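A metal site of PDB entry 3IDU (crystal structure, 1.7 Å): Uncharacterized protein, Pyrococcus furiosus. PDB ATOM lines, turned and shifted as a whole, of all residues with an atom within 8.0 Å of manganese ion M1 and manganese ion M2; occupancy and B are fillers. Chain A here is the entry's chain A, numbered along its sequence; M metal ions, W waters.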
ATOM      1  N   PRO A  17      29.551 -36.386  25.091  1.00  0.00           N
ATOM      2  CA  PRO A  17      29.530 -35.414  26.180  1.00  0.00           C
ATOM      3  C   PRO A  17      28.057 -35.037  26.324  1.00  0.00           C
ATOM      4  O   PRO A  17      27.225 -35.482  25.538  1.00  0.00           O
ATOM      5  CB  PRO A  17      30.367 -34.252  25.621  1.00  0.00           C
ATOM      6  CG  PRO A  17      30.092 -34.299  24.148  1.00  0.00           C
ATOM      7  CD  PRO A  17      30.088 -35.799  23.850  1.00  0.00           C
ATOM      8  N   ASP A  18      27.723 -34.273  27.357  1.00  0.00           N
ATOM      9  CA  ASP A  18      26.356 -33.789  27.518  1.00  0.00           C
ATOM     10  C   ASP A  18      26.410 -32.520  28.341  1.00  0.00           C
ATOM     11  O   ASP A  18      26.573 -32.544  29.557  1.00  0.00           O
ATOM     12  CB  ASP A  18      25.395 -34.774  28.197  1.00  0.00           C
ATOM     13  CG  ASP A  18      23.965 -34.257  28.205  1.00  0.00           C
ATOM     14  OD1 ASP A  18      23.727 -33.197  27.591  1.00  0.00           O
ATOM     15  OD2 ASP A  18      23.064 -34.892  28.802  1.00  0.00           O
ATOM     16  N   LEU A  19      26.292 -31.415  27.635  1.00  0.00           N
ATOM     17  CA  LEU A  19      26.336 -30.110  28.259  1.00  0.00           C
ATOM     18  C   LEU A  19      24.999 -29.712  28.842  1.00  0.00           C
ATOM     19  O   LEU A  19      23.955 -29.945  28.239  1.00  0.00           O
ATOM     20  CB  LEU A  19      26.759 -29.085  27.209  1.00  0.00           C
ATOM     21  CG  LEU A  19      28.130 -29.366  26.599  1.00  0.00           C
ATOM     22  CD1 LEU A  19      28.312 -28.575  25.312  1.00  0.00           C
ATOM     23  CD2 LEU A  19      29.206 -28.997  27.613  1.00  0.00           C
ATOM     24  N   THR A  20      25.026 -29.093  30.015  1.00  0.00           N
ATOM     25  CA  THR A  20      23.804 -28.637  30.654  1.00  0.00           C
ATOM     26  C   THR A  20      24.104 -27.328  31.373  1.00  0.00           C
ATOM     27  O   THR A  20      25.267 -27.033  31.684  1.00  0.00           O
ATOM     28  CB  THR A  20      23.292 -29.674  31.674  1.00  0.00           C
ATOM     29  OG1 THR A  20      21.921 -29.376  31.989  1.00  0.00           O
ATOM     30  CG2 THR A  20      24.108 -29.624  32.942  1.00  0.00           C
ATOM     31  N   VAL A  21      23.065 -26.548  31.648  1.00  0.00           N
ATOM     32  CA  VAL A  21      23.232 -25.282  32.339  1.00  0.00           C
ATOM     33  C   VAL A  21      22.123 -25.041  33.357  1.00  0.00           C
ATOM     34  O   VAL A  21      20.996 -25.493  33.184  1.00  0.00           O
ATOM     35  CB  VAL A  21      23.235 -24.081  31.356  1.00  0.00           C
ATOM     36  CG1 VAL A  21      24.491 -24.102  30.500  1.00  0.00           C
ATOM     37  CG2 VAL A  21      21.989 -24.129  30.489  1.00  0.00           C
ATOM     38  N   LYS A  42      27.726 -27.869  33.230  1.00  0.00           N
ATOM     39  CA  LYS A  42      28.278 -29.185  33.487  1.00  0.00           C
ATOM     40  C   LYS A  42      28.357 -30.055  32.241  1.00  0.00           C
ATOM     41  O   LYS A  42      27.620 -29.836  31.278  1.00  0.00           O
ATOM     42  CB  LYS A  42      27.423 -29.909  34.532  1.00  0.00           C
ATOM     43  CG  LYS A  42      27.019 -29.010  35.698  1.00  0.00           C
ATOM     44  CD  LYS A  42      25.956 -29.628  36.595  1.00  0.00           C
ATOM     45  CE  LYS A  42      26.525 -30.720  37.492  1.00  0.00           C
ATOM     46  NZ  LYS A  42      25.534 -31.155  38.521  1.00  0.00           N
ATOM     47  N   ASN A  43      29.261 -31.016  32.268  1.00  0.00           N
ATOM     48  CA  ASN A  43      29.393 -31.979  31.185  1.00  0.00           C
ATOM     49  C   ASN A  43      29.107 -33.303  31.869  1.00  0.00           C
ATOM     50  O   ASN A  43      29.952 -33.820  32.604  1.00  0.00           O
ATOM     51  CB  ASN A  43      30.807 -32.017  30.611  1.00  0.00           C
ATOM     52  CG  ASN A  43      30.960 -33.059  29.515  1.00  0.00           C
ATOM     53  OD1 ASN A  43      29.988 -33.707  29.133  1.00  0.00           O
ATOM     54  ND2 ASN A  43      32.179 -33.202  29.001  1.00  0.00           N
ATOM     55  N   LEU A  44      27.908 -33.836  31.651  1.00  0.00           N
ATOM     56  CA  LEU A  44      27.515 -35.091  32.278  1.00  0.00           C
ATOM     57  C   LEU A  44      28.103 -36.301  31.554  1.00  0.00           C
ATOM     58  O   LEU A  44      28.041 -37.420  32.073  1.00  0.00           O
ATOM     59  CB  LEU A  44      26.000 -35.215  32.288  1.00  0.00           C
ATOM     60  CG  LEU A  44      25.218 -34.004  32.811  1.00  0.00           C
ATOM     61  CD1 LEU A  44      23.726 -34.233  32.624  1.00  0.00           C
ATOM     62  CD2 LEU A  44      25.561 -33.769  34.268  1.00  0.00           C
ATOM     63  N   THR A  52      33.251 -24.569  24.030  1.00  0.00           N
ATOM     64  CA  THR A  52      31.842 -24.338  23.741  1.00  0.00           C
ATOM     65  C   THR A  52      31.459 -22.986  24.306  1.00  0.00           C
ATOM     66  O   THR A  52      32.110 -22.470  25.223  1.00  0.00           O
ATOM     67  CB  THR A  52      30.907 -25.423  24.330  1.00  0.00           C
ATOM     68  OG1 THR A  52      29.589 -25.254  23.798  1.00  0.00           O
ATOM     69  CG2 THR A  52      30.848 -25.327  25.840  1.00  0.00           C
ATOM     70  N   VAL A  96      24.003 -23.146  26.484  1.00  0.00           N
ATOM     71  CA  VAL A  96      25.326 -23.687  26.237  1.00  0.00           C
ATOM     72  C   VAL A  96      25.239 -24.407  24.893  1.00  0.00           C
ATOM     73  O   VAL A  96      24.266 -25.099  24.601  1.00  0.00           O
ATOM     74  CB  VAL A  96      25.799 -24.620  27.389  1.00  0.00           C
ATOM     75  CG1 VAL A  96      24.834 -25.786  27.555  1.00  0.00           C
ATOM     76  CG2 VAL A  96      27.207 -25.110  27.103  1.00  0.00           C
ATOM     77  N   ASP A  97      26.271 -24.214  24.067  1.00  0.00           N
ATOM     78  CA  ASP A  97      26.318 -24.768  22.715  1.00  0.00           C
ATOM     79  C   ASP A  97      25.035 -24.454  21.969  1.00  0.00           C
ATOM     80  O   ASP A  97      24.434 -25.328  21.349  1.00  0.00           O
ATOM     81  CB  ASP A  97      26.547 -26.270  22.705  1.00  0.00           C
ATOM     82  CG  ASP A  97      26.792 -26.797  21.293  1.00  0.00           C
ATOM     83  OD1 ASP A  97      27.363 -26.026  20.490  1.00  0.00           O
ATOM     84  OD2 ASP A  97      26.421 -27.952  20.986  1.00  0.00           O
ATOM     85  N   GLU A  98      24.617 -23.199  22.023  1.00  0.00           N
ATOM     86  CA  GLU A  98      23.395 -22.797  21.341  1.00  0.00           C
ATOM     87  C   GLU A  98      23.491 -23.020  19.837  1.00  0.00           C
ATOM     88  O   GLU A  98      22.476 -23.274  19.187  1.00  0.00           O
ATOM     89  CB  GLU A  98      23.108 -21.328  21.635  1.00  0.00           C
ATOM     90  CG  GLU A  98      21.651 -20.961  21.508  1.00  0.00           C
ATOM     91  CD  GLU A  98      21.398 -19.498  21.781  1.00  0.00           C
ATOM     92  OE1 GLU A  98      21.985 -18.967  22.752  1.00  0.00           O
ATOM     93  OE2 GLU A  98      20.616 -18.884  21.036  1.00  0.00           O
ATOM     94  N   GLU A  99      24.691 -22.928  19.285  1.00  0.00           N
ATOM     95  CA  GLU A  99      24.904 -23.126  17.843  1.00  0.00           C
ATOM     96  C   GLU A  99      24.978 -24.611  17.510  1.00  0.00           C
ATOM     97  O   GLU A  99      25.160 -24.995  16.351  1.00  0.00           O
ATOM     98  CB  GLU A  99      26.201 -22.451  17.391  1.00  0.00           C
ATOM     99  CG  GLU A  99      27.415 -22.808  18.246  1.00  0.00           C
ATOM    100  CD  GLU A  99      27.628 -21.820  19.381  1.00  0.00           C
ATOM    101  OE1 GLU A  99      28.022 -20.668  19.091  1.00  0.00           O
ATOM    102  OE2 GLU A  99      27.402 -22.191  20.551  1.00  0.00           O
ATOM    103  N   ASN A 100      24.818 -25.432  18.535  1.00  0.00           N
ATOM    104  CA  ASN A 100      24.863 -26.880  18.440  1.00  0.00           C
ATOM    105  C   ASN A 100      25.981 -27.403  17.546  1.00  0.00           C
ATOM    106  O   ASN A 100      25.745 -28.000  16.488  1.00  0.00           O
ATOM    107  CB  ASN A 100      23.520 -27.444  17.992  1.00  0.00           C
ATOM    108  CG  ASN A 100      23.474 -28.955  18.060  1.00  0.00           C
ATOM    109  OD1 ASN A 100      24.098 -29.576  18.943  1.00  0.00           O
ATOM    110  ND2 ASN A 100      22.727 -29.563  17.143  1.00  0.00           N
ATOM    111  N   THR A 101      27.209 -27.174  17.986  1.00  0.00           N
ATOM    112  CA  THR A 101      28.385 -27.642  17.267  1.00  0.00           C
ATOM    113  C   THR A 101      28.980 -28.848  17.998  1.00  0.00           C
ATOM    114  O   THR A 101      30.006 -29.394  17.580  1.00  0.00           O
ATOM    115  CB  THR A 101      29.439 -26.509  17.157  1.00  0.00           C
ATOM    116  OG1 THR A 101      29.725 -25.994  18.464  1.00  0.00           O
ATOM    117  CG2 THR A 101      28.917 -25.383  16.280  1.00  0.00           C
ATOM    118  N   VAL A 102      28.330 -29.249  19.080  1.00  0.00           N
ATOM    119  CA  VAL A 102      28.779 -30.402  19.876  1.00  0.00           C
ATOM    120  C   VAL A 102      27.685 -31.467  19.940  1.00  0.00           C
ATOM    121  O   VAL A 102      26.595 -31.196  20.417  1.00  0.00           O
ATOM    122  CB  VAL A 102      29.132 -29.985  21.319  1.00  0.00           C
ATOM    123  CG1 VAL A 102      29.657 -31.179  22.093  1.00  0.00           C
ATOM    124  CG2 VAL A 102      30.156 -28.853  21.316  1.00  0.00           C
ATOM    125  N   VAL A 103      27.976 -32.661  19.440  1.00  0.00           N
ATOM    126  CA  VAL A 103      27.000 -33.757  19.485  1.00  0.00           C
ATOM    127  C   VAL A 103      26.977 -34.280  20.902  1.00  0.00           C
ATOM    128  O   VAL A 103      27.992 -34.730  21.415  1.00  0.00           O
ATOM    129  CB  VAL A 103      27.379 -34.898  18.511  1.00  0.00           C
ATOM    130  CG1 VAL A 103      26.432 -36.088  18.691  1.00  0.00           C
ATOM    131  CG2 VAL A 103      27.297 -34.383  17.070  1.00  0.00           C
ATOM    132  N   GLU A 104      25.807 -34.233  21.535  1.00  0.00           N
ATOM    133  CA  GLU A 104      25.663 -34.681  22.923  1.00  0.00           C
ATOM    134  C   GLU A 104      24.589 -35.733  23.100  1.00  0.00           C
ATOM    135  O   GLU A 104      23.822 -36.039  22.185  1.00  0.00           O
ATOM    136  CB  GLU A 104      25.273 -33.514  23.832  1.00  0.00           C
ATOM    137  CG  GLU A 104      26.095 -32.250  23.696  1.00  0.00           C
ATOM    138  CD  GLU A 104      25.313 -31.028  24.178  1.00  0.00           C
ATOM    139  OE1 GLU A 104      24.725 -31.088  25.272  1.00  0.00           O
ATOM    140  OE2 GLU A 104      25.274 -30.019  23.453  1.00  0.00           O
ATOM    141  N   LEU A 105      24.528 -36.256  24.314  1.00  0.00           N
ATOM    142  CA  LEU A 105      23.539 -37.251  24.686  1.00  0.00           C
ATOM    143  C   LEU A 105      22.150 -36.603  24.693  1.00  0.00           C
ATOM    144  O   LEU A 105      21.139 -37.266  24.519  1.00  0.00           O
ATOM    145  CB  LEU A 105      23.833 -37.798  26.076  1.00  0.00           C
ATOM    146  CG  LEU A 105      25.190 -38.433  26.315  1.00  0.00           C
ATOM    147  CD1 LEU A 105      25.396 -38.664  27.803  1.00  0.00           C
ATOM    148  CD2 LEU A 105      25.291 -39.748  25.546  1.00  0.00           C
ATOM    149  N   ASN A 106      22.116 -35.291  24.900  1.00  0.00           N
ATOM    150  CA  ASN A 106      20.854 -34.557  24.959  1.00  0.00           C
ATOM    151  C   ASN A 106      21.088 -33.108  24.551  1.00  0.00           C
ATOM    152  O   ASN A 106      21.980 -32.438  25.079  1.00  0.00           O
ATOM    153  CB  ASN A 106      20.294 -34.628  26.390  1.00  0.00           C
ATOM    154  CG  ASN A 106      18.908 -34.032  26.517  1.00  0.00           C
ATOM    155  OD1 ASN A 106      18.365 -33.462  25.580  1.00  0.00           O
ATOM    156  ND2 ASN A 106      18.320 -34.167  27.707  1.00  0.00           N
ATOM    157  N   GLU A 107      20.310 -32.631  23.578  1.00  0.00           N
ATOM    158  CA  GLU A 107      20.454 -31.248  23.121  1.00  0.00           C
ATOM    159  C   GLU A 107      19.306 -30.413  23.697  1.00  0.00           C
ATOM    160  O   GLU A 107      19.229 -29.199  23.475  1.00  0.00           O
ATOM    161  CB  GLU A 107      20.406 -31.175  21.578  1.00  0.00           C
ATOM    162  CG  GLU A 107      21.223 -32.241  20.842  1.00  0.00           C
ATOM    163  CD  GLU A 107      22.723 -32.086  21.011  1.00  0.00           C
ATOM    164  OE1 GLU A 107      23.472 -33.000  20.560  1.00  0.00           O
ATOM    165  OE2 GLU A 107      23.176 -31.062  21.582  1.00  0.00           O
ATOM    166  N   ASN A 108      18.426 -31.068  24.447  1.00  0.00           N
ATOM    167  CA  ASN A 108      17.273 -30.381  25.013  1.00  0.00           C
ATOM    168  C   ASN A 108      17.414 -29.965  26.482  1.00  0.00           C
ATOM    169  O   ASN A 108      16.445 -29.521  27.095  1.00  0.00           O
ATOM    170  CB  ASN A 108      16.018 -31.251  24.817  1.00  0.00           C
ATOM    171  CG  ASN A 108      15.816 -31.651  23.362  1.00  0.00           C
ATOM    172  OD1 ASN A 108      16.030 -32.813  22.989  1.00  0.00           O
ATOM    173  ND2 ASN A 108      15.423 -30.683  22.537  1.00  0.00           N
ATOM    174  N   ASN A 109      18.615 -30.102  27.033  1.00  0.00           N
ATOM    175  CA  ASN A 109      18.863 -29.693  28.420  1.00  0.00           C
ATOM    176  C   ASN A 109      19.970 -28.643  28.401  1.00  0.00           C
ATOM    177  O   ASN A 109      20.703 -28.463  29.384  1.00  0.00           O
ATOM    178  CB  ASN A 109      19.275 -30.895  29.283  1.00  0.00           C
ATOM    179  CG  ASN A 109      20.542 -31.581  28.787  1.00  0.00           C
ATOM    180  OD1 ASN A 109      21.047 -31.272  27.709  1.00  0.00           O
ATOM    181  ND2 ASN A 109      21.058 -32.524  29.570  1.00  0.00           N
ATOM    182  N   ASN A 110      20.078 -27.950  27.278  1.00  0.00           N
ATOM    183  CA  ASN A 110      21.098 -26.924  27.090  1.00  0.00           C
ATOM    184  C   ASN A 110      20.600 -25.514  27.361  1.00  0.00           C
ATOM    185  O   ASN A 110      21.314 -24.550  27.097  1.00  0.00           O
ATOM    186  CB  ASN A 110      21.646 -27.003  25.667  1.00  0.00           C
ATOM    187  CG  ASN A 110      22.500 -28.229  25.431  1.00  0.00           C
ATOM    188  OD1 ASN A 110      22.120 -29.339  25.784  1.00  0.00           O
ATOM    189  ND2 ASN A 110      23.658 -28.036  24.826  1.00  0.00           N
ATOM    190  N   VAL A 111      19.378 -25.384  27.871  1.00  0.00           N
ATOM    191  CA  VAL A 111      18.818 -24.070  28.152  1.00  0.00           C
ATOM    192  C   VAL A 111      18.234 -23.976  29.554  1.00  0.00           C
ATOM    193  O   VAL A 111      17.483 -24.854  29.987  1.00  0.00           O
ATOM    194  CB  VAL A 111      17.715 -23.719  27.141  1.00  0.00           C
ATOM    195  CG1 VAL A 111      17.128 -22.351  27.452  1.00  0.00           C
ATOM    196  CG2 VAL A 111      18.270 -23.739  25.718  1.00  0.00           C
HETATM  197 MN    MN M   1      22.957 -31.191  26.656  1.00  0.00          MN
HETATM  198 MN    MN M   2      25.022 -29.693  21.295  1.00  0.00          MN
HETATM  199  O   HOH W   1      23.586 -27.862  21.466  1.00  0.00           O
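Manganese ion M2 is bound by OE2 of Glu 104 (2.2 Å), OD2 of Asp 97 (2.3 Å), OE2 of Glu 107 (2.3 Å), water W1 (2.3 Å), O of Val 102 (2.3 Å) and OD1 of Asn 100 (2.5 Å).
N of Asp 97 sits close to OG1 of Thr 52, 3.5 Å away. N of Leu 44 lies within hydrogen-bond range of O of Asp 18. The backbone carbonyl oxygen (O) of Asn 109 lies within hydrogen-bond range of the side-chain hydroxyl (OG1) of Thr 20. The side-chain carboxylate (OD1) of Asp 97 lies within hydrogen-bond range of the backbone NH (N) of Thr 101. The backbone NH (N) of Asn 108 lies within hydrogen-bond range of the side-chain amide oxygen (OD1) of Asn 106 (2.6 Å). The side-chain amide nitrogen (ND2) of Asn 110 is in hydrogen-bond range of the backbone carbonyl oxygen (O) of Val 96. OD1 of Asn 43 is in hydrogen-bond range of N of Asp 18 (2.9 Å).
Of the 25 residues printed, 6 come within 4 Å of manganese ion M1. The nearest printed residue that does not touch manganese ion M1 is Glu 107 (4.3 Å).
Five residues have an atom within 4 Å of manganese ion M2: Asp 97, Asn 100, Val 102, Glu 104 and Glu 107. The nearest printed residue that does not touch manganese ion M2 is Asn 110 (4.1 Å).
Manganese ion M1 is bound by the side-chain amide oxygen (OD1) of Asn 109 (2.2 Å), the side-chain amide oxygen (OD1) of Asn 110 (2.2 Å), the backbone carbonyl oxygen (O) of Asn 106 (2.2 Å), the side-chain carboxylate (OE1) of Glu 104 (2.2 Å), the backbone carbonyl oxygen (O) of Leu 19 (2.2 Å) and the side-chain carboxylate (OD1) of Asp 18 (2.3 Å). Manganese ion M1 has six donor atoms within binding distance.
Water W1 lies within hydrogen-bond range of O of Asp 97 and ND2 of Asn 110.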
